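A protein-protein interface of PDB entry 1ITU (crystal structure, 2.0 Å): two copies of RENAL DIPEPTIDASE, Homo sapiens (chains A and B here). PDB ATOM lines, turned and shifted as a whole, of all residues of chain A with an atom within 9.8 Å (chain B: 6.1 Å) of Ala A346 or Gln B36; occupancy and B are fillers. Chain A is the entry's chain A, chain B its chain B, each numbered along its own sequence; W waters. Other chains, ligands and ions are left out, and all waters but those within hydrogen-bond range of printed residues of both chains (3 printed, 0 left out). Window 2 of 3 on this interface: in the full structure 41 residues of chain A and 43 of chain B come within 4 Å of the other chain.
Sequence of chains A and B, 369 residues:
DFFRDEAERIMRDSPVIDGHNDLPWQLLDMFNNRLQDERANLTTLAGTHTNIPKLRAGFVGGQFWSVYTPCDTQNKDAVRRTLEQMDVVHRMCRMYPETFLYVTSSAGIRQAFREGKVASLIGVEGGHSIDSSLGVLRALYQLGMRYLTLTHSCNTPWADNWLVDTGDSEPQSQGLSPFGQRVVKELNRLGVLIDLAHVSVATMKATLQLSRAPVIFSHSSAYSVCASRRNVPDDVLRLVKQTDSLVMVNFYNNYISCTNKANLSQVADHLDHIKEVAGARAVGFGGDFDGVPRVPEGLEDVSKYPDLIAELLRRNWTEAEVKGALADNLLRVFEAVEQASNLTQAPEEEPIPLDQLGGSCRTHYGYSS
The backbone carbonyl oxygen (O) of Pro A347 is in hydrogen-bond range of the side-chain amide nitrogen (NE2) of Gln B36, at 3.4 Å. OE2 of Glu A349 sits at hydrogen-bond distance from N of Leu B35 (3.0 Å). N of Gln B36 is in hydrogen-bond range of OE1 of Glu A349. The guanidinium group of Arg B91 lies within salt-bridge range of the side-chain carboxylate of Glu A349 (2.8 Å).
O of Asn B33 lies within hydrogen-bond range of NH1 of Arg B91 (2.7 Å). The guanidinium group of Arg A138 is in hydrogen-bond range of the backbone carbonyl oxygen of Glu A348 (2.9 Å). The guanidinium group (NH2) of Arg A138 is in salt-bridge range of the side-chain carboxylate (OE1) of Glu A186, at 2.9 Å. OE2 of Glu A350 lies within salt-bridge range of NE of Arg A182 (3.8 Å).
Arg A138 touches Arg B91. NE2 of Gln B36 touches CB of Ala A346, at 3.6 Å. Pro A347 touches Arg B91. O of Asn B33 touches OE2 of Glu A349, at 3.7 Å. Arg B34 touches Glu A349 (C to OE1, 3.2 Å). CG of Glu A350 touches NH1 of Arg B34 (3.6 Å).
Printed residues of chain B within 4 Å of Arg A138: Arg B91 (3.5 Å). Printed residues of chain B within 4 Å of Ala A346: Gln B36. Of the printed residues of chain B, Pro A347 touches Gln B36 (3.4 Å) and Arg B91 (3.95 Å). Printed residues of chain B within 4 Å of Glu A350: Arg B34. Of the printed residues of chain A, Gln B36 touches Ala A346, Pro A347 and Glu A349. The nearest residue of chain B that does not touch Ala A346 is Met B95 (5.7 Å). The nearest printed residue of chain B that does not touch Glu A349 is Asp B37 (4.1 Å).
Printed residues of chain B that touch a printed residue of chain A: Asn B33, Arg B34, Leu B35, Gln B36 and Arg B91. Hydrophobic or aromatic side chains of chain B that line the printed part of chain A: Leu B35. Among the printed residues, 10 pairs touch across the chains. Among the printed residues, Asp or Glu carboxylates within 4 Å of a Lys or Arg side-chain nitrogen of the other chain: Glu A349 with Arg B91.
No position is printed for both chains. Of the 10 pairs that touch across the chains among the printed residues, none has its exchanged pair printed and touching as well.
Water W2 lies within hydrogen-bond range of NE2 of Gln B36, O of Pro A347 and OE2 of Glu A349. Water W3 bridges the side-chain carboxylate (OE1) of Glu A349 and the guanidinium group (NE) of Arg B34. Water W1 lies within hydrogen-bond range of NE2 of Gln B36 and O of Pro A347.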
ATOM      1  N   LEU A 134      10.133  26.909 -13.374  1.00  0.00           N
ATOM      2  CA  LEU A 134      10.959  27.859 -12.645  1.00  0.00           C
ATOM      3  C   LEU A 134      11.324  29.054 -13.536  1.00  0.00           C
ATOM      4  O   LEU A 134      11.576  30.143 -13.036  1.00  0.00           O
ATOM      5  CB  LEU A 134      12.201  27.160 -12.082  1.00  0.00           C
ATOM      6  CG  LEU A 134      11.863  26.095 -11.021  1.00  0.00           C
ATOM      7  CD1 LEU A 134      12.934  25.015 -10.953  1.00  0.00           C
ATOM      8  CD2 LEU A 134      11.647  26.753  -9.668  1.00  0.00           C
ATOM      9  N   ARG A 138      10.566  33.008 -12.685  1.00  0.00           N
ATOM     10  CA  ARG A 138      11.521  34.104 -12.801  1.00  0.00           C
ATOM     11  C   ARG A 138      11.001  35.197 -13.736  1.00  0.00           C
ATOM     12  O   ARG A 138      11.226  36.383 -13.494  1.00  0.00           O
ATOM     13  CB  ARG A 138      12.877  33.591 -13.279  1.00  0.00           C
ATOM     14  CG  ARG A 138      13.670  32.901 -12.179  1.00  0.00           C
ATOM     15  CD  ARG A 138      15.076  32.540 -12.627  1.00  0.00           C
ATOM     16  NE  ARG A 138      15.090  31.417 -13.557  1.00  0.00           N
ATOM     17  CZ  ARG A 138      15.052  30.140 -13.187  1.00  0.00           C
ATOM     18  NH1 ARG A 138      15.080  29.184 -14.110  1.00  0.00           N
ATOM     19  NH2 ARG A 138      14.973  29.810 -11.898  1.00  0.00           N
ATOM     20  N   ARG A 182      11.736  23.215  -4.089  1.00  0.00           N
ATOM     21  CA  ARG A 182      12.662  23.990  -4.919  1.00  0.00           C
ATOM     22  C   ARG A 182      12.030  25.340  -5.288  1.00  0.00           C
ATOM     23  O   ARG A 182      12.721  26.355  -5.343  1.00  0.00           O
ATOM     24  CB  ARG A 182      13.091  23.197  -6.161  1.00  0.00           C
ATOM     25  CG  ARG A 182      13.946  21.992  -5.812  1.00  0.00           C
ATOM     26  CD  ARG A 182      14.764  21.507  -7.000  1.00  0.00           C
ATOM     27  NE  ARG A 182      13.959  20.959  -8.084  1.00  0.00           N
ATOM     28  CZ  ARG A 182      13.364  19.773  -8.051  1.00  0.00           C
ATOM     29  NH1 ARG A 182      12.664  19.345  -9.100  1.00  0.00           N
ATOM     30  NH2 ARG A 182      13.442  19.020  -6.958  1.00  0.00           N
ATOM     31  N   LYS A 185      12.472  27.574  -2.408  1.00  0.00           N
ATOM     32  CA  LYS A 185      13.868  28.022  -2.361  1.00  0.00           C
ATOM     33  C   LYS A 185      14.127  29.145  -3.390  1.00  0.00           C
ATOM     34  O   LYS A 185      14.829  30.125  -3.109  1.00  0.00           O
ATOM     35  CB  LYS A 185      14.807  26.839  -2.602  1.00  0.00           C
ATOM     36  CG  LYS A 185      16.279  27.222  -2.621  1.00  0.00           C
ATOM     37  CD  LYS A 185      17.203  26.009  -2.602  1.00  0.00           C
ATOM     38  CE  LYS A 185      18.652  26.434  -2.398  1.00  0.00           C
ATOM     39  NZ  LYS A 185      19.508  25.252  -2.099  1.00  0.00           N
ATOM     40  N   GLU A 186      13.552  29.001  -4.580  1.00  0.00           N
ATOM     41  CA  GLU A 186      13.702  30.013  -5.624  1.00  0.00           C
ATOM     42  C   GLU A 186      12.975  31.295  -5.187  1.00  0.00           C
ATOM     43  O   GLU A 186      13.482  32.402  -5.368  1.00  0.00           O
ATOM     44  CB  GLU A 186      13.141  29.484  -6.950  1.00  0.00           C
ATOM     45  CG  GLU A 186      13.311  30.434  -8.144  1.00  0.00           C
ATOM     46  CD  GLU A 186      14.764  30.641  -8.589  1.00  0.00           C
ATOM     47  OE1 GLU A 186      14.978  31.428  -9.528  1.00  0.00           O
ATOM     48  OE2 GLU A 186      15.698  30.038  -8.013  1.00  0.00           O
ATOM     49  N   LEU A 187      11.787  31.147  -4.602  1.00  0.00           N
ATOM     50  CA  LEU A 187      11.051  32.316  -4.127  1.00  0.00           C
ATOM     51  C   LEU A 187      11.909  33.076  -3.109  1.00  0.00           C
ATOM     52  O   LEU A 187      12.005  34.301  -3.174  1.00  0.00           O
ATOM     53  CB  LEU A 187       9.686  31.914  -3.545  1.00  0.00           C
ATOM     54  CG  LEU A 187       8.596  31.460  -4.534  1.00  0.00           C
ATOM     55  CD1 LEU A 187       7.374  30.911  -3.812  1.00  0.00           C
ATOM     56  CD2 LEU A 187       8.181  32.623  -5.423  1.00  0.00           C
ATOM     57  N   ASN A 188      12.597  32.351  -2.215  1.00  0.00           N
ATOM     58  CA  ASN A 188      13.473  32.998  -1.229  1.00  0.00           C
ATOM     59  C   ASN A 188      14.660  33.686  -1.900  1.00  0.00           C
ATOM     60  O   ASN A 188      14.984  34.817  -1.548  1.00  0.00           O
ATOM     61  CB  ASN A 188      14.037  32.005  -0.195  1.00  0.00           C
ATOM     62  CG  ASN A 188      12.997  31.491   0.787  1.00  0.00           C
ATOM     63  OD1 ASN A 188      13.220  30.463   1.422  1.00  0.00           O
ATOM     64  ND2 ASN A 188      11.876  32.197   0.935  1.00  0.00           N
ATOM     65  N   ARG A 189      15.332  33.017  -2.843  1.00  0.00           N
ATOM     66  CA  ARG A 189      16.488  33.652  -3.486  1.00  0.00           C
ATOM     67  C   ARG A 189      16.096  34.890  -4.285  1.00  0.00           C
ATOM     68  O   ARG A 189      16.805  35.886  -4.269  1.00  0.00           O
ATOM     69  CB  ARG A 189      17.330  32.673  -4.336  1.00  0.00           C
ATOM     70  CG  ARG A 189      16.659  32.103  -5.567  1.00  0.00           C
ATOM     71  CD  ARG A 189      17.696  31.576  -6.590  1.00  0.00           C
ATOM     72  NE  ARG A 189      18.524  32.653  -7.102  1.00  0.00           N
ATOM     73  CZ  ARG A 189      18.263  33.378  -8.186  1.00  0.00           C
ATOM     74  NH1 ARG A 189      19.094  34.346  -8.524  1.00  0.00           N
ATOM     75  NH2 ARG A 189      17.211  33.124  -8.956  1.00  0.00           N
ATOM     76  N   LEU A 190      14.923  34.851  -4.904  1.00  0.00           N
ATOM     77  CA  LEU A 190      14.446  35.975  -5.692  1.00  0.00           C
ATOM     78  C   LEU A 190      14.034  37.182  -4.870  1.00  0.00           C
ATOM     79  O   LEU A 190      14.234  38.312  -5.286  1.00  0.00           O
ATOM     80  CB  LEU A 190      13.275  35.540  -6.569  1.00  0.00           C
ATOM     81  CG  LEU A 190      13.659  34.780  -7.842  1.00  0.00           C
ATOM     82  CD1 LEU A 190      12.420  34.228  -8.515  1.00  0.00           C
ATOM     83  CD2 LEU A 190      14.439  35.715  -8.777  1.00  0.00           C
ATOM     84  N   ARG A 212      13.222  30.434   4.273  1.00  0.00           N
ATOM     85  CA  ARG A 212      14.393  31.059   4.881  1.00  0.00           C
ATOM     86  C   ARG A 212      14.090  32.529   5.208  1.00  0.00           C
ATOM     87  O   ARG A 212      14.932  33.265   5.734  1.00  0.00           O
ATOM     88  CB  ARG A 212      15.545  30.922   3.872  1.00  0.00           C
ATOM     89  CG  ARG A 212      16.897  31.473   4.257  1.00  0.00           C
ATOM     90  CD  ARG A 212      17.953  31.014   3.237  1.00  0.00           C
ATOM     91  NE  ARG A 212      17.653  31.405   1.851  1.00  0.00           N
ATOM     92  CZ  ARG A 212      17.713  32.653   1.394  1.00  0.00           C
ATOM     93  NH1 ARG A 212      17.438  32.918   0.119  1.00  0.00           N
ATOM     94  NH2 ARG A 212      18.039  33.638   2.225  1.00  0.00           N
ATOM     95  N   SER A 341      17.044  37.491  -0.028  1.00  0.00           N
ATOM     96  CA  SER A 341      17.280  37.179  -1.437  1.00  0.00           C
ATOM     97  C   SER A 341      18.785  37.179  -1.711  1.00  0.00           C
ATOM     98  O   SER A 341      19.550  37.771  -0.951  1.00  0.00           O
ATOM     99  CB  SER A 341      16.593  38.213  -2.327  1.00  0.00           C
ATOM    100  OG  SER A 341      17.261  39.461  -2.264  1.00  0.00           O
ATOM    101  N   ASN A 342      19.203  36.511  -2.786  1.00  0.00           N
ATOM    102  CA  ASN A 342      20.616  36.431  -3.171  1.00  0.00           C
ATOM    103  C   ASN A 342      20.724  36.502  -4.699  1.00  0.00           C
ATOM    104  O   ASN A 342      20.384  35.549  -5.390  1.00  0.00           O
ATOM    105  CB  ASN A 342      21.229  35.117  -2.661  1.00  0.00           C
ATOM    106  CG  ASN A 342      22.758  35.081  -2.770  1.00  0.00           C
ATOM    107  OD1 ASN A 342      23.408  34.263  -2.120  1.00  0.00           O
ATOM    108  ND2 ASN A 342      23.332  35.962  -3.583  1.00  0.00           N
ATOM    109  N   LEU A 343      21.212  37.627  -5.213  1.00  0.00           N
ATOM    110  CA  LEU A 343      21.361  37.836  -6.659  1.00  0.00           C
ATOM    111  C   LEU A 343      22.467  37.002  -7.295  1.00  0.00           C
ATOM    112  O   LEU A 343      22.411  36.676  -8.485  1.00  0.00           O
ATOM    113  CB  LEU A 343      21.624  39.317  -6.966  1.00  0.00           C
ATOM    114  CG  LEU A 343      20.476  40.325  -6.809  1.00  0.00           C
ATOM    115  CD1 LEU A 343      19.269  39.845  -7.612  1.00  0.00           C
ATOM    116  CD2 LEU A 343      20.108  40.512  -5.331  1.00  0.00           C
ATOM    117  N   THR A 344      23.470  36.669  -6.492  1.00  0.00           N
ATOM    118  CA  THR A 344      24.610  35.890  -6.939  1.00  0.00           C
ATOM    119  C   THR A 344      24.380  34.385  -6.890  1.00  0.00           C
ATOM    120  O   THR A 344      25.065  33.628  -7.577  1.00  0.00           O
ATOM    121  CB  THR A 344      25.845  36.252  -6.114  1.00  0.00           C
ATOM    122  OG1 THR A 344      26.020  37.676  -6.152  1.00  0.00           O
ATOM    123  CG2 THR A 344      27.098  35.574  -6.676  1.00  0.00           C
ATOM    124  N   GLN A 345      23.419  33.951  -6.078  1.00  0.00           N
ATOM    125  CA  GLN A 345      23.102  32.530  -5.965  1.00  0.00           C
ATOM    126  C   GLN A 345      22.559  32.056  -7.318  1.00  0.00           C
ATOM    127  O   GLN A 345      21.741  32.738  -7.942  1.00  0.00           O
ATOM    128  CB  GLN A 345      22.051  32.305  -4.868  1.00  0.00           C
ATOM    129  CG  GLN A 345      21.845  30.851  -4.426  1.00  0.00           C
ATOM    130  CD  GLN A 345      20.718  30.690  -3.396  1.00  0.00           C
ATOM    131  OE1 GLN A 345      19.913  29.758  -3.475  1.00  0.00           O
ATOM    132  NE2 GLN A 345      20.654  31.607  -2.434  1.00  0.00           N
ATOM    133  N   ALA A 346      23.069  30.923  -7.791  1.00  0.00           N
ATOM    134  CA  ALA A 346      22.636  30.346  -9.052  1.00  0.00           C
ATOM    135  C   ALA A 346      21.162  29.980  -8.955  1.00  0.00           C
ATOM    136  O   ALA A 346      20.729  29.372  -7.977  1.00  0.00           O
ATOM    137  CB  ALA A 346      23.458  29.115  -9.369  1.00  0.00           C
ATOM    138  N   PRO A 347      20.369  30.353  -9.977  1.00  0.00           N
ATOM    139  CA  PRO A 347      18.931  30.071 -10.019  1.00  0.00           C
ATOM    140  C   PRO A 347      18.615  28.586  -9.990  1.00  0.00           C
ATOM    141  O   PRO A 347      19.383  27.773 -10.494  1.00  0.00           O
ATOM    142  CB  PRO A 347      18.510  30.671 -11.367  1.00  0.00           C
ATOM    143  CG  PRO A 347      19.500  31.771 -11.576  1.00  0.00           C
ATOM    144  CD  PRO A 347      20.786  31.131 -11.156  1.00  0.00           C
ATOM    145  N   GLU A 348      17.482  28.232  -9.394  1.00  0.00           N
ATOM    146  CA  GLU A 348      17.053  26.842  -9.361  1.00  0.00           C
ATOM    147  C   GLU A 348      16.695  26.445 -10.797  1.00  0.00           C
ATOM    148  O   GLU A 348      15.920  27.127 -11.463  1.00  0.00           O
ATOM    149  CB  GLU A 348      15.830  26.686  -8.458  1.00  0.00           C
ATOM    150  CG  GLU A 348      16.128  26.881  -6.977  1.00  0.00           C
ATOM    151  CD  GLU A 348      17.018  25.781  -6.407  1.00  0.00           C
ATOM    152  OE1 GLU A 348      16.584  24.608  -6.401  1.00  0.00           O
ATOM    153  OE2 GLU A 348      18.152  26.093  -5.972  1.00  0.00           O
ATOM    154  N   GLU A 349      17.261  25.350 -11.274  1.00  0.00           N
ATOM    155  CA  GLU A 349      16.995  24.916 -12.635  1.00  0.00           C
ATOM    156  C   GLU A 349      16.654  23.440 -12.781  1.00  0.00           C
ATOM    157  O   GLU A 349      16.572  22.939 -13.896  1.00  0.00           O
ATOM    158  CB  GLU A 349      18.172  25.278 -13.544  1.00  0.00           C
ATOM    159  CG  GLU A 349      19.440  24.492 -13.245  1.00  0.00           C
ATOM    160  CD  GLU A 349      20.589  24.860 -14.153  1.00  0.00           C
ATOM    161  OE1 GLU A 349      21.525  24.043 -14.283  1.00  0.00           O
ATOM    162  OE2 GLU A 349      20.565  25.964 -14.727  1.00  0.00           O
ATOM    163  N   GLU A 350      16.492  22.726 -11.669  1.00  0.00           N
ATOM    164  CA  GLU A 350      16.109  21.322 -11.761  1.00  0.00           C
ATOM    165  C   GLU A 350      14.595  21.339 -11.953  1.00  0.00           C
ATOM    166  O   GLU A 350      13.827  21.604 -11.012  1.00  0.00           O
ATOM    167  CB  GLU A 350      16.509  20.530 -10.510  1.00  0.00           C
ATOM    168  CG  GLU A 350      16.305  19.014 -10.663  1.00  0.00           C
ATOM    169  CD  GLU A 350      16.680  18.210  -9.419  1.00  0.00           C
ATOM    170  OE1 GLU A 350      16.591  16.963  -9.475  1.00  0.00           O
ATOM    171  OE2 GLU A 350      17.056  18.815  -8.385  1.00  0.00           O
ATOM    172  N   ASN B  33      17.625  23.195 -20.457  1.00  0.00           N
ATOM    173  CA  ASN B  33      17.995  24.511 -19.939  1.00  0.00           C
ATOM    174  C   ASN B  33      18.759  24.527 -18.613  1.00  0.00           C
ATOM    175  O   ASN B  33      18.739  25.523 -17.884  1.00  0.00           O
ATOM    176  CB  ASN B  33      16.775  25.430 -19.891  1.00  0.00           C
ATOM    177  CG  ASN B  33      16.301  25.824 -21.275  1.00  0.00           C
ATOM    178  OD1 ASN B  33      17.091  25.871 -22.223  1.00  0.00           O
ATOM    179  ND2 ASN B  33      15.012  26.109 -21.402  1.00  0.00           N
ATOM    180  N   ARG B  34      19.448  23.425 -18.315  1.00  0.00           N
ATOM    181  CA  ARG B  34      20.247  23.324 -17.102  1.00  0.00           C
ATOM    182  C   ARG B  34      21.654  23.817 -17.434  1.00  0.00           C
ATOM    183  O   ARG B  34      22.530  23.037 -17.817  1.00  0.00           O
ATOM    184  CB  ARG B  34      20.263  21.883 -16.589  1.00  0.00           C
ATOM    185  CG  ARG B  34      18.861  21.343 -16.373  1.00  0.00           C
ATOM    186  CD  ARG B  34      18.869  19.962 -15.790  1.00  0.00           C
ATOM    187  NE  ARG B  34      19.354  19.983 -14.415  1.00  0.00           N
ATOM    188  CZ  ARG B  34      19.007  19.104 -13.476  1.00  0.00           C
ATOM    189  NH1 ARG B  34      19.505  19.216 -12.249  1.00  0.00           N
ATOM    190  NH2 ARG B  34      18.167  18.113 -13.757  1.00  0.00           N
ATOM    191  N   LEU B  35      21.850  25.126 -17.285  1.00  0.00           N
ATOM    192  CA  LEU B  35      23.118  25.781 -17.591  1.00  0.00           C
ATOM    193  C   LEU B  35      24.278  25.399 -16.680  1.00  0.00           C
ATOM    194  O   LEU B  35      25.447  25.639 -17.013  1.00  0.00           O
ATOM    195  CB  LEU B  35      22.928  27.300 -17.610  1.00  0.00           C
ATOM    196  CG  LEU B  35      21.896  27.817 -18.618  1.00  0.00           C
ATOM    197  CD1 LEU B  35      21.856  29.322 -18.575  1.00  0.00           C
ATOM    198  CD2 LEU B  35      22.231  27.330 -20.019  1.00  0.00           C
ATOM    199  N   GLN B  36      23.954  24.789 -15.542  1.00  0.00           N
ATOM    200  CA  GLN B  36      24.967  24.361 -14.588  1.00  0.00           C
ATOM    201  C   GLN B  36      25.573  23.030 -14.970  1.00  0.00           C
ATOM    202  O   GLN B  36      26.614  22.651 -14.435  1.00  0.00           O
ATOM    203  CB  GLN B  36      24.396  24.296 -13.175  1.00  0.00           C
ATOM    204  CG  GLN B  36      24.116  25.645 -12.579  1.00  0.00           C
ATOM    205  CD  GLN B  36      23.434  25.536 -11.241  1.00  0.00           C
ATOM    206  OE1 GLN B  36      23.937  24.881 -10.325  1.00  0.00           O
ATOM    207  NE2 GLN B  36      22.271  26.164 -11.118  1.00  0.00           N
ATOM    208  N   ASP B  37      24.887  22.295 -15.839  1.00  0.00           N
ATOM    209  CA  ASP B  37      25.373  21.015 -16.354  1.00  0.00           C
ATOM    210  C   ASP B  37      26.758  21.369 -16.920  1.00  0.00           C
ATOM    211  O   ASP B  37      26.886  22.308 -17.718  1.00  0.00           O
ATOM    212  CB  ASP B  37      24.429  20.543 -17.479  1.00  0.00           C
ATOM    213  CG  ASP B  37      24.745  19.134 -17.992  1.00  0.00           C
ATOM    214  OD1 ASP B  37      25.929  18.819 -18.234  1.00  0.00           O
ATOM    215  OD2 ASP B  37      23.795  18.345 -18.190  1.00  0.00           O
ATOM    216  N   GLU B  38      27.806  20.684 -16.469  1.00  0.00           N
ATOM    217  CA  GLU B  38      29.147  21.015 -16.954  1.00  0.00           C
ATOM    218  C   GLU B  38      29.331  20.816 -18.452  1.00  0.00           C
ATOM    219  O   GLU B  38      30.183  21.449 -19.070  1.00  0.00           O
ATOM    220  CB  GLU B  38      30.232  20.312 -16.136  1.00  0.00           C
ATOM    221  CG  GLU B  38      30.257  20.737 -14.644  1.00  0.00           C
ATOM    222  CD  GLU B  38      30.612  22.223 -14.387  1.00  0.00           C
ATOM    223  OE1 GLU B  38      31.250  22.495 -13.342  1.00  0.00           O
ATOM    224  OE2 GLU B  38      30.245  23.119 -15.190  1.00  0.00           O
ATOM    225  N   ARG B  39      28.482  19.978 -19.033  1.00  0.00           N
ATOM    226  CA  ARG B  39      28.492  19.710 -20.458  1.00  0.00           C
ATOM    227  C   ARG B  39      27.927  20.942 -21.194  1.00  0.00           C
ATOM    228  O   ARG B  39      28.167  21.132 -22.382  1.00  0.00           O
ATOM    229  CB  ARG B  39      27.644  18.464 -20.718  1.00  0.00           C
ATOM    230  CG  ARG B  39      27.232  18.223 -22.149  1.00  0.00           C
ATOM    231  CD  ARG B  39      28.358  17.679 -23.025  1.00  0.00           C
ATOM    232  NE  ARG B  39      27.994  17.769 -24.436  1.00  0.00           N
ATOM    233  CZ  ARG B  39      28.405  18.735 -25.251  1.00  0.00           C
ATOM    234  NH1 ARG B  39      29.216  19.694 -24.804  1.00  0.00           N
ATOM    235  NH2 ARG B  39      27.939  18.784 -26.492  1.00  0.00           N
ATOM    236  N   ALA B  40      27.226  21.799 -20.451  1.00  0.00           N
ATOM    237  CA  ALA B  40      26.614  23.014 -20.979  1.00  0.00           C
ATOM    238  C   ALA B  40      27.465  24.264 -20.771  1.00  0.00           C
ATOM    239  O   ALA B  40      27.010  25.377 -21.065  1.00  0.00           O
ATOM    240  CB  ALA B  40      25.234  23.217 -20.352  1.00  0.00           C
ATOM    241  N   ARG B  91      19.600  34.180 -18.029  1.00  0.00           N
ATOM    242  CA  ARG B  91      20.562  33.468 -17.180  1.00  0.00           C
ATOM    243  C   ARG B  91      21.938  33.296 -17.812  1.00  0.00           C
ATOM    244  O   ARG B  91      22.955  33.321 -17.123  1.00  0.00           O
ATOM    245  CB  ARG B  91      19.996  32.112 -16.772  1.00  0.00           C
ATOM    246  CG  ARG B  91      18.711  32.224 -15.978  1.00  0.00           C
ATOM    247  CD  ARG B  91      18.358  30.925 -15.309  1.00  0.00           C
ATOM    248  NE  ARG B  91      17.801  29.934 -16.217  1.00  0.00           N
ATOM    249  CZ  ARG B  91      18.258  28.694 -16.349  1.00  0.00           C
ATOM    250  NH1 ARG B  91      17.655  27.861 -17.182  1.00  0.00           N
ATOM    251  NH2 ARG B  91      19.345  28.302 -15.692  1.00  0.00           N
ATOM    252  N   MET B  95      25.296  34.454 -16.272  1.00  0.00           N
ATOM    253  CA  MET B  95      26.287  33.404 -16.023  1.00  0.00           C
ATOM    254  C   MET B  95      27.660  33.680 -16.670  1.00  0.00           C
ATOM    255  O   MET B  95      28.694  33.265 -16.134  1.00  0.00           O
ATOM    256  CB  MET B  95      25.761  32.028 -16.461  1.00  0.00           C
ATOM    257  CG  MET B  95      26.670  30.881 -16.022  1.00  0.00           C
ATOM    258  SD  MET B  95      26.066  29.211 -16.333  1.00  0.00           S
ATOM    259  CE  MET B  95      25.014  28.928 -14.869  1.00  0.00           C
HETATM  260  O   HOH W   1      20.966  25.888  -8.591  1.00  0.00           O
HETATM  261  O   HOH W   2      21.171  27.855 -12.524  1.00  0.00           O
HETATM  262  O   HOH W   3      21.657  21.719 -13.382  1.00  0.00           O
